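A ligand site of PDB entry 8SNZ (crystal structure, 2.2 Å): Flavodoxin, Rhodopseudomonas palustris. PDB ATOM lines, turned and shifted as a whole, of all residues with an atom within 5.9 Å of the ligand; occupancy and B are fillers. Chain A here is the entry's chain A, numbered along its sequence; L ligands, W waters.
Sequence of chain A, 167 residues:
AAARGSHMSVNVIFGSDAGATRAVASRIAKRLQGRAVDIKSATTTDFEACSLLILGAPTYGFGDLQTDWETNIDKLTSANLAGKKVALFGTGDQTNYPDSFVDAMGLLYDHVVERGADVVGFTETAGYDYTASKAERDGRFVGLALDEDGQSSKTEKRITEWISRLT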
ATOM      1  N   GLY A  15     -37.568   2.638  -2.509  1.00  0.00           N
ATOM      2  CA  GLY A  15     -36.691   1.875  -1.650  1.00  0.00           C
ATOM      3  C   GLY A  15     -35.288   2.433  -1.748  1.00  0.00           C
ATOM      4  O   GLY A  15     -34.905   3.019  -2.761  1.00  0.00           O
ATOM      5  N   SER A  16     -34.516   2.261  -0.681  1.00  0.00           N
ATOM      6  CA  SER A  16     -33.173   2.829  -0.646  1.00  0.00           C
ATOM      7  C   SER A  16     -32.349   2.134   0.428  1.00  0.00           C
ATOM      8  O   SER A  16     -32.853   1.825   1.504  1.00  0.00           O
ATOM      9  CB  SER A  16     -33.213   4.343  -0.373  1.00  0.00           C
ATOM     10  OG  SER A  16     -32.002   4.965  -0.735  1.00  0.00           O
ATOM     11  N   ASP A  17     -31.075   1.888   0.103  1.00  0.00           N
ATOM     12  CA  ASP A  17     -30.105   1.343   1.038  1.00  0.00           C
ATOM     13  C   ASP A  17     -29.038   2.343   1.434  1.00  0.00           C
ATOM     14  O   ASP A  17     -28.653   2.393   2.609  1.00  0.00           O
ATOM     15  CB  ASP A  17     -29.423   0.101   0.438  1.00  0.00           C
ATOM     16  CG  ASP A  17     -30.247  -1.149   0.590  1.00  0.00           C
ATOM     17  OD1 ASP A  17     -31.402  -1.060   1.070  1.00  0.00           O
ATOM     18  OD2 ASP A  17     -29.739  -2.236   0.233  1.00  0.00           O
ATOM     19  N   ALA A  18     -28.553   3.146   0.497  1.00  0.00           N
ATOM     20  CA  ALA A  18     -27.519   4.139   0.773  1.00  0.00           C
ATOM     21  C   ALA A  18     -27.985   5.578   0.536  1.00  0.00           C
ATOM     22  O   ALA A  18     -27.148   6.476   0.456  1.00  0.00           O
ATOM     23  CB  ALA A  18     -26.277   3.859  -0.084  1.00  0.00           C
ATOM     24  N   GLY A  19     -29.292   5.816   0.423  1.00  0.00           N
ATOM     25  CA  GLY A  19     -29.832   7.163   0.396  1.00  0.00           C
ATOM     26  C   GLY A  19     -29.946   7.815  -0.969  1.00  0.00           C
ATOM     27  O   GLY A  19     -30.558   8.887  -1.064  1.00  0.00           O
ATOM     28  N   ALA A  20     -29.397   7.208  -2.018  1.00  0.00           N
ATOM     29  CA  ALA A  20     -29.418   7.848  -3.336  1.00  0.00           C
ATOM     30  C   ALA A  20     -30.834   7.887  -3.905  1.00  0.00           C
ATOM     31  O   ALA A  20     -31.309   8.932  -4.367  1.00  0.00           O
ATOM     32  CB  ALA A  20     -28.470   7.139  -4.292  1.00  0.00           C
ATOM     33  N   THR A  21     -31.533   6.750  -3.880  1.00  0.00           N
ATOM     34  CA  THR A  21     -32.912   6.721  -4.378  1.00  0.00           C
ATOM     35  C   THR A  21     -33.848   7.505  -3.462  1.00  0.00           C
ATOM     36  O   THR A  21     -34.838   8.064  -3.938  1.00  0.00           O
ATOM     37  CB  THR A  21     -33.397   5.274  -4.515  1.00  0.00           C
ATOM     38  OG1 THR A  21     -32.327   4.455  -5.021  1.00  0.00           O
ATOM     39  CG2 THR A  21     -34.576   5.200  -5.463  1.00  0.00           C
ATOM     40  N   ARG A  22     -33.544   7.561  -2.168  1.00  0.00           N
ATOM     41  CA  ARG A  22     -34.390   8.296  -1.232  1.00  0.00           C
ATOM     42  C   ARG A  22     -34.362   9.785  -1.534  1.00  0.00           C
ATOM     43  O   ARG A  22     -35.398  10.461  -1.460  1.00  0.00           O
ATOM     44  CB  ARG A  22     -33.935   8.027   0.204  1.00  0.00           C
ATOM     45  CG  ARG A  22     -34.484   8.995   1.236  1.00  0.00           C
ATOM     46  CD  ARG A  22     -34.358   8.437   2.646  1.00  0.00           C
ATOM     47  NE  ARG A  22     -32.967   8.215   3.023  1.00  0.00           N
ATOM     48  CZ  ARG A  22     -32.448   7.028   3.301  1.00  0.00           C
ATOM     49  NH1 ARG A  22     -33.182   5.926   3.263  1.00  0.00           N
ATOM     50  NH2 ARG A  22     -31.167   6.945   3.634  1.00  0.00           N
ATOM     51  N   PRO A  58     -33.581   1.161  -6.433  1.00  0.00           N
ATOM     52  CA  PRO A  58     -32.254   0.813  -6.945  1.00  0.00           C
ATOM     53  C   PRO A  58     -32.161  -0.681  -7.204  1.00  0.00           C
ATOM     54  O   PRO A  58     -32.989  -1.476  -6.741  1.00  0.00           O
ATOM     55  CB  PRO A  58     -31.327   1.238  -5.805  1.00  0.00           C
ATOM     56  CG  PRO A  58     -32.153   1.052  -4.569  1.00  0.00           C
ATOM     57  CD  PRO A  58     -33.601   1.234  -4.962  1.00  0.00           C
ATOM     58  N   THR A  59     -31.149  -1.052  -7.962  1.00  0.00           N
ATOM     59  CA  THR A  59     -30.877  -2.457  -8.260  1.00  0.00           C
ATOM     60  C   THR A  59     -29.718  -2.930  -7.394  1.00  0.00           C
ATOM     61  O   THR A  59     -28.651  -2.303  -7.372  1.00  0.00           O
ATOM     62  CB  THR A  59     -30.560  -2.659  -9.742  1.00  0.00           C
ATOM     63  OG1 THR A  59     -31.597  -2.074 -10.531  1.00  0.00           O
ATOM     64  CG2 THR A  59     -30.487  -4.141 -10.056  1.00  0.00           C
ATOM     65  N   TYR A  60     -29.935  -4.022  -6.668  1.00  0.00           N
ATOM     66  CA  TYR A  60     -28.917  -4.541  -5.752  1.00  0.00           C
ATOM     67  C   TYR A  60     -28.733  -6.032  -5.933  1.00  0.00           C
ATOM     68  O   TYR A  60     -29.248  -6.627  -6.892  1.00  0.00           O
ATOM     69  CB  TYR A  60     -29.299  -4.229  -4.309  1.00  0.00           C
ATOM     70  CG  TYR A  60     -28.791  -2.894  -3.812  1.00  0.00           C
ATOM     71  CD1 TYR A  60     -27.480  -2.741  -3.383  1.00  0.00           C
ATOM     72  CD2 TYR A  60     -29.637  -1.785  -3.762  1.00  0.00           C
ATOM     73  CE1 TYR A  60     -27.020  -1.524  -2.930  1.00  0.00           C
ATOM     74  CE2 TYR A  60     -29.176  -0.569  -3.309  1.00  0.00           C
ATOM     75  CZ  TYR A  60     -27.868  -0.443  -2.894  1.00  0.00           C
ATOM     76  OH  TYR A  60     -27.417   0.775  -2.443  1.00  0.00           O
ATOM     77  N   GLY A  61     -28.004  -6.657  -5.012  1.00  0.00           N
ATOM     78  CA  GLY A  61     -27.759  -8.087  -5.051  1.00  0.00           C
ATOM     79  C   GLY A  61     -27.150  -8.551  -6.358  1.00  0.00           C
ATOM     80  O   GLY A  61     -25.979  -8.284  -6.638  1.00  0.00           O
ATOM     81  N   PHE A  62     -27.948  -9.246  -7.157  1.00  0.00           N
ATOM     82  CA  PHE A  62     -27.520  -9.775  -8.444  1.00  0.00           C
ATOM     83  C   PHE A  62     -28.570  -9.433  -9.501  1.00  0.00           C
ATOM     84  O   PHE A  62     -29.197 -10.301 -10.106  1.00  0.00           O
ATOM     85  CB  PHE A  62     -27.270 -11.278  -8.348  1.00  0.00           C
ATOM     86  CG  PHE A  62     -26.485 -11.673  -7.122  1.00  0.00           C
ATOM     87  CD1 PHE A  62     -25.098 -11.676  -7.149  1.00  0.00           C
ATOM     88  CD2 PHE A  62     -27.126 -12.024  -5.953  1.00  0.00           C
ATOM     89  CE1 PHE A  62     -24.369 -12.025  -6.030  1.00  0.00           C
ATOM     90  CE2 PHE A  62     -26.408 -12.371  -4.826  1.00  0.00           C
ATOM     91  CZ  PHE A  62     -25.029 -12.372  -4.865  1.00  0.00           C
ATOM     92  N   GLY A  63     -28.749  -8.139  -9.713  1.00  0.00           N
ATOM     93  CA  GLY A  63     -29.814  -7.661 -10.581  1.00  0.00           C
ATOM     94  C   GLY A  63     -31.192  -7.829  -9.989  1.00  0.00           C
ATOM     95  O   GLY A  63     -32.153  -8.086 -10.724  1.00  0.00           O
ATOM     96  N   ASP A  64     -31.318  -7.684  -8.673  1.00  0.00           N
ATOM     97  CA  ASP A  64     -32.578  -7.890  -7.961  1.00  0.00           C
ATOM     98  C   ASP A  64     -33.137  -6.554  -7.501  1.00  0.00           C
ATOM     99  O   ASP A  64     -32.454  -5.522  -7.491  1.00  0.00           O
ATOM    100  CB  ASP A  64     -32.376  -8.818  -6.767  1.00  0.00           C
ATOM    101  CG  ASP A  64     -31.711 -10.123  -7.142  1.00  0.00           C
ATOM    102  OD1 ASP A  64     -32.275 -10.863  -7.975  1.00  0.00           O
ATOM    103  OD2 ASP A  64     -30.613 -10.401  -6.612  1.00  0.00           O
ATOM    104  N   GLN A  66     -34.322  -3.934  -4.662  1.00  0.00           N
ATOM    105  CA  GLN A  66     -33.827  -3.618  -3.341  1.00  0.00           C
ATOM    106  C   GLN A  66     -34.572  -4.446  -2.291  1.00  0.00           C
ATOM    107  O   GLN A  66     -35.767  -4.733  -2.449  1.00  0.00           O
ATOM    108  CB  GLN A  66     -33.982  -2.115  -3.071  1.00  0.00           C
ATOM    109  CG  GLN A  66     -33.432  -1.657  -1.732  1.00  0.00           C
ATOM    110  CD  GLN A  66     -34.537  -1.401  -0.729  1.00  0.00           C
ATOM    111  OE1 GLN A  66     -35.722  -1.501  -1.046  1.00  0.00           O
ATOM    112  NE2 GLN A  66     -34.148  -1.073   0.502  1.00  0.00           N
ATOM    113  N   THR A  91     -32.596   3.816 -10.122  1.00  0.00           N
ATOM    114  CA  THR A  91     -31.213   4.217  -9.905  1.00  0.00           C
ATOM    115  C   THR A  91     -30.308   3.027 -10.159  1.00  0.00           C
ATOM    116  O   THR A  91     -30.632   1.893  -9.776  1.00  0.00           O
ATOM    117  CB  THR A  91     -30.992   4.748  -8.485  1.00  0.00           C
ATOM    118  OG1 THR A  91     -31.766   3.985  -7.557  1.00  0.00           O
ATOM    119  CG2 THR A  91     -31.412   6.212  -8.403  1.00  0.00           C
ATOM    120  N   GLY A  92     -29.176   3.265 -10.808  1.00  0.00           N
ATOM    121  CA  GLY A  92     -28.300   2.175 -11.148  1.00  0.00           C
ATOM    122  C   GLY A  92     -26.880   2.632 -11.399  1.00  0.00           C
ATOM    123  O   GLY A  92     -26.535   3.802 -11.179  1.00  0.00           O
ATOM    124  N   ASP A  93     -26.060   1.692 -11.853  1.00  0.00           N
ATOM    125  CA  ASP A  93     -24.648   1.929 -12.133  1.00  0.00           C
ATOM    126  C   ASP A  93     -24.329   1.196 -13.435  1.00  0.00           C
ATOM    127  O   ASP A  93     -24.058  -0.010 -13.431  1.00  0.00           O
ATOM    128  CB  ASP A  93     -23.765   1.437 -10.983  1.00  0.00           C
ATOM    129  CG  ASP A  93     -22.311   1.842 -11.131  1.00  0.00           C
ATOM    130  OD1 ASP A  93     -21.941   2.376 -12.195  1.00  0.00           O
ATOM    131  OD2 ASP A  93     -21.540   1.624 -10.173  1.00  0.00           O
ATOM    132  N   GLN A  94     -24.365   1.929 -14.550  1.00  0.00           N
ATOM    133  CA  GLN A  94     -24.137   1.314 -15.854  1.00  0.00           C
ATOM    134  C   GLN A  94     -22.668   0.970 -16.093  1.00  0.00           C
ATOM    135  O   GLN A  94     -22.381   0.132 -16.952  1.00  0.00           O
ATOM    136  CB  GLN A  94     -24.643   2.230 -16.974  1.00  0.00           C
ATOM    137  CG  GLN A  94     -23.723   3.398 -17.302  1.00  0.00           C
ATOM    138  CD  GLN A  94     -24.490   4.610 -17.798  1.00  0.00           C
ATOM    139  OE1 GLN A  94     -24.587   4.854 -18.995  1.00  0.00           O
ATOM    140  NE2 GLN A  94     -25.030   5.386 -16.860  1.00  0.00           N
ATOM    141  N   TYR A  97     -22.244  -2.342 -13.656  1.00  0.00           N
ATOM    142  CA  TYR A  97     -23.268  -3.363 -13.903  1.00  0.00           C
ATOM    143  C   TYR A  97     -23.917  -3.123 -15.266  1.00  0.00           C
ATOM    144  O   TYR A  97     -25.121  -2.865 -15.358  1.00  0.00           O
ATOM    145  CB  TYR A  97     -24.307  -3.361 -12.786  1.00  0.00           C
ATOM    146  CG  TYR A  97     -23.705  -3.383 -11.384  1.00  0.00           C
ATOM    147  CD1 TYR A  97     -23.389  -2.205 -10.728  1.00  0.00           C
ATOM    148  CD2 TYR A  97     -23.457  -4.592 -10.739  1.00  0.00           C
ATOM    149  CE1 TYR A  97     -22.845  -2.217  -9.459  1.00  0.00           C
ATOM    150  CE2 TYR A  97     -22.916  -4.614  -9.472  1.00  0.00           C
ATOM    151  CZ  TYR A  97     -22.605  -3.431  -8.837  1.00  0.00           C
ATOM    152  OH  TYR A  97     -22.064  -3.453  -7.569  1.00  0.00           O
ATOM    153  N   SER A 100     -26.928  -5.601 -16.129  1.00  0.00           N
ATOM    154  CA  SER A 100     -28.090  -5.592 -15.259  1.00  0.00           C
ATOM    155  C   SER A 100     -28.454  -4.165 -14.874  1.00  0.00           C
ATOM    156  O   SER A 100     -28.793  -3.876 -13.723  1.00  0.00           O
ATOM    157  CB  SER A 100     -27.863  -6.450 -14.011  1.00  0.00           C
ATOM    158  OG  SER A 100     -26.651  -6.097 -13.370  1.00  0.00           O
ATOM    159  N   PHE A 101     -28.368  -3.259 -15.842  1.00  0.00           N
ATOM    160  CA  PHE A 101     -28.571  -1.841 -15.571  1.00  0.00           C
ATOM    161  C   PHE A 101     -30.043  -1.560 -15.259  1.00  0.00           C
ATOM    162  O   PHE A 101     -30.926  -1.927 -16.034  1.00  0.00           O
ATOM    163  CB  PHE A 101     -28.112  -1.014 -16.766  1.00  0.00           C
ATOM    164  CG  PHE A 101     -28.180   0.471 -16.544  1.00  0.00           C
ATOM    165  CD1 PHE A 101     -27.661   1.035 -15.392  1.00  0.00           C
ATOM    166  CD2 PHE A 101     -28.752   1.299 -17.491  1.00  0.00           C
ATOM    167  CE1 PHE A 101     -27.720   2.398 -15.183  1.00  0.00           C
ATOM    168  CE2 PHE A 101     -28.818   2.665 -17.294  1.00  0.00           C
ATOM    169  CZ  PHE A 101     -28.304   3.208 -16.136  1.00  0.00           C
ATOM    170  N   VAL A 102     -30.272  -0.886 -14.132  1.00  0.00           N
ATOM    171  CA  VAL A 102     -31.589  -0.590 -13.553  1.00  0.00           C
ATOM    172  C   VAL A 102     -32.586  -1.713 -13.829  1.00  0.00           C
ATOM    173  O   VAL A 102     -33.731  -1.458 -14.227  1.00  0.00           O
ATOM    174  CB  VAL A 102     -32.131   0.777 -14.039  1.00  0.00           C
ATOM    175  CG1 VAL A 102     -31.307   1.911 -13.447  1.00  0.00           C
ATOM    176  CG2 VAL A 102     -32.170   0.887 -15.560  1.00  0.00           C
ATOM    177  N   ASP A 103     -32.163  -2.949 -13.595  1.00  0.00           N
ATOM    178  CA  ASP A 103     -33.057  -4.095 -13.772  1.00  0.00           C
ATOM    179  C   ASP A 103     -34.242  -4.032 -12.828  1.00  0.00           C
ATOM    180  O   ASP A 103     -35.326  -4.527 -13.154  1.00  0.00           O
ATOM    181  CB  ASP A 103     -32.289  -5.402 -13.584  1.00  0.00           C
ATOM    182  CG  ASP A 103     -31.662  -5.904 -14.861  1.00  0.00           C
ATOM    183  OD1 ASP A 103     -31.684  -5.169 -15.871  1.00  0.00           O
ATOM    184  OD2 ASP A 103     -31.150  -7.046 -14.866  1.00  0.00           O
ATOM    185  N   GLU A 148     -26.522   7.668 -10.461  1.00  0.00           N
ATOM    186  CA  GLU A 148     -25.878   8.585  -9.530  1.00  0.00           C
ATOM    187  C   GLU A 148     -24.429   8.222  -9.231  1.00  0.00           C
ATOM    188  O   GLU A 148     -23.760   8.974  -8.520  1.00  0.00           O
ATOM    189  CB  GLU A 148     -26.677   8.650  -8.227  1.00  0.00           C
ATOM    190  CG  GLU A 148     -27.932   9.501  -8.316  1.00  0.00           C
ATOM    191  CD  GLU A 148     -27.615  10.984  -8.431  1.00  0.00           C
ATOM    192  OE1 GLU A 148     -27.434  11.632  -7.384  1.00  0.00           O
ATOM    193  OE2 GLU A 148     -27.548  11.488  -9.566  1.00  0.00           O
ATOM    194  N   ASP A 149     -23.940   7.104  -9.760  1.00  0.00           N
ATOM    195  CA  ASP A 149     -22.581   6.662  -9.508  1.00  0.00           C
ATOM    196  C   ASP A 149     -21.596   7.191 -10.549  1.00  0.00           C
ATOM    197  O   ASP A 149     -20.548   7.739 -10.192  1.00  0.00           O
ATOM    198  CB  ASP A 149     -22.526   5.135  -9.451  1.00  0.00           C
ATOM    199  CG  ASP A 149     -23.254   4.569  -8.254  1.00  0.00           C
ATOM    200  OD1 ASP A 149     -23.162   5.173  -7.157  1.00  0.00           O
ATOM    201  OD2 ASP A 149     -23.919   3.523  -8.395  1.00  0.00           O
HETATM  202  N1  LIG L   1     -26.852  -0.928 -10.308  1.00  0.00           N
HETATM  203  C1  LIG L   1     -27.408  -1.415 -11.456  1.00  0.00           C
HETATM  204  O1  LIG L   1     -27.794  -0.664 -12.369  1.00  0.00           O
HETATM  205  N2  LIG L   1     -27.549  -2.778 -11.642  1.00  0.00           N
HETATM  206  C2  LIG L   1     -27.175  -3.761 -10.740  1.00  0.00           C
HETATM  207  O2  LIG L   1     -27.361  -4.949 -11.014  1.00  0.00           O
HETATM  208  C3  LIG L   1     -26.583  -3.240  -9.519  1.00  0.00           C
HETATM  209  N3  LIG L   1     -26.194  -4.092  -8.618  1.00  0.00           N
HETATM  210  C4  LIG L   1     -25.607  -3.601  -7.463  1.00  0.00           C
HETATM  211  C5  LIG L   1     -25.166  -4.503  -6.498  1.00  0.00           C
HETATM  212  C6  LIG L   1     -24.570  -4.057  -5.326  1.00  0.00           C
HETATM  213  C7  LIG L   1     -24.120  -5.063  -4.290  1.00  0.00           C
HETATM  214  C8  LIG L   1     -24.400  -2.682  -5.114  1.00  0.00           C
HETATM  215  C9  LIG L   1     -23.732  -2.169  -3.859  1.00  0.00           C
HETATM  216  C10 LIG L   1     -24.841  -1.772  -6.068  1.00  0.00           C
HETATM  217  C11 LIG L   1     -25.439  -2.228  -7.241  1.00  0.00           C
HETATM  218  N4  LIG L   1     -25.888  -1.340  -8.240  1.00  0.00           N
HETATM  219  C12 LIG L   1     -26.458  -1.803  -9.399  1.00  0.00           C
HETATM  220  C13 LIG L   1     -25.778   0.121  -8.059  1.00  0.00           C
HETATM  221  C14 LIG L   1     -26.852   0.717  -7.162  1.00  0.00           C
HETATM  222  O3  LIG L   1     -28.154   0.320  -7.620  1.00  0.00           O
HETATM  223  C15 LIG L   1     -26.750   2.241  -7.179  1.00  0.00           C
HETATM  224  O4  LIG L   1     -25.571   2.631  -6.479  1.00  0.00           O
HETATM  225  C16 LIG L   1     -27.955   2.941  -6.550  1.00  0.00           C
HETATM  226  O5  LIG L   1     -27.897   4.339  -6.827  1.00  0.00           O
HETATM  227  C17 LIG L   1     -28.068   2.708  -5.063  1.00  0.00           C
HETATM  228  O6  LIG L   1     -29.248   3.373  -4.566  1.00  0.00           O
HETATM  229  P1  LIG L   1     -29.399   3.632  -2.964  1.00  0.00           P
HETATM  230  O7  LIG L   1     -28.232   4.493  -2.576  1.00  0.00           O
HETATM  231  O8  LIG L   1     -29.367   2.264  -2.318  1.00  0.00           O
HETATM  232  O9  LIG L   1     -30.737   4.323  -2.791  1.00  0.00           O
HETATM  233  O   HOH W   1     -25.340   5.704  -5.512  1.00  0.00           O
HETATM  234  O   HOH W   2     -27.260   5.522  -9.124  1.00  0.00           O
HETATM  235  O   HOH W   3     -26.097  -7.119  -9.642  1.00  0.00           O
HETATM  236  O   HOH W   4     -21.622  -5.825  -6.519  1.00  0.00           O
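Merely in contact with the ligand: Pro 58, Gly 61, Gly 63, Thr 91, Gly 92, Tyr 97 and Phe 101. Hydrophobic or aromatic side chains within 4 Å of the ligand: Ala 18, Ala 20, Pro 58, Tyr 60, Tyr 97 and Phe 101. Of the 27 residues printed, 19 come within 4 Å of the ligand.
The side-chain hydroxyl (OH) of Tyr 60 lies within hydrogen-bond range of an oxygen (O8) of the ligand. O9 of the ligand lies within hydrogen-bond range of OG of Ser 16 (2.5 Å). O of Ser 100 sits at hydrogen-bond distance from N2 of the ligand, 2.7 Å away. The side-chain hydroxyl (OG) of Ser 100 sits at hydrogen-bond distance from an oxygen (O2) of the ligand (2.7 Å). N of Thr 59 lies within hydrogen-bond range of O3 of the ligand. O of Thr 59 sits at hydrogen-bond distance from O3 of the ligand. OD2 of Asp 149 is in hydrogen-bond range of O4 of the ligand (2.7 Å). O9 of the ligand is in hydrogen-bond range of N of Thr 21 (2.8 Å). An oxygen (O9) of the ligand lies within hydrogen-bond range of the side-chain hydroxyl (OG1) of Thr 21 (2.7 Å). An oxygen (O1) of the ligand is in hydrogen-bond range of the backbone NH (N) of Asp 93. An oxygen (O8) of the ligand lies within hydrogen-bond range of the backbone NH of Asp 17, 3.0 Å away. O7 of the ligand sits at hydrogen-bond distance from N of Ala 20. N of Val 102 lies within hydrogen-bond range of O1 of the ligand (3.0 Å). The backbone NH (N) of Ala 18 lies within hydrogen-bond range of an oxygen (O8) of the ligand (3.1 Å). N of Gly 19 sits at hydrogen-bond distance from O7 of the ligand.
The backbone NH of Gly 19 lies within hydrogen-bond range of the side-chain hydroxyl of Ser 16, at 3.1 Å. The side-chain hydroxyl (OG) of Ser 16 is in hydrogen-bond range of the backbone NH (N) of Arg 22. The backbone carbonyl oxygen of Ser 16 lies within hydrogen-bond range of the side-chain amide nitrogen of Gln 66, at 3.3 Å. The backbone NH (N) of Thr 59 lies within hydrogen-bond range of the backbone carbonyl oxygen (O) of Thr 91. The backbone NH of Asp 103 sits at hydrogen-bond distance from the side-chain hydroxyl of Thr 59 (3.2 Å). The side-chain hydroxyl of Thr 21 lies within hydrogen-bond range of the side-chain hydroxyl of Thr 91. The side-chain carboxylate (OD1) of Asp 17 lies within hydrogen-bond range of the side-chain amide nitrogen (NE2) of Gln 66. O of Pro 58 sits at hydrogen-bond distance from N of Gln 66.
Water W2 lies within hydrogen-bond range of the backbone NH (N) of Glu 148 (2.6 Å), an oxygen (O5) of the ligand (2.7 Å) and the backbone carbonyl oxygen (O) of Gly 92 (2.8 Å). Water W3 lies within hydrogen-bond range of N of Gly 63 (2.8 Å), O2 of the ligand (2.9 Å) and O of Gly 61 (3.2 Å). Water W1 lies within hydrogen-bond range of the side-chain carboxylate of Asp 149 (2.8 Å) and an oxygen (O5) of the ligand (3.2 Å).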
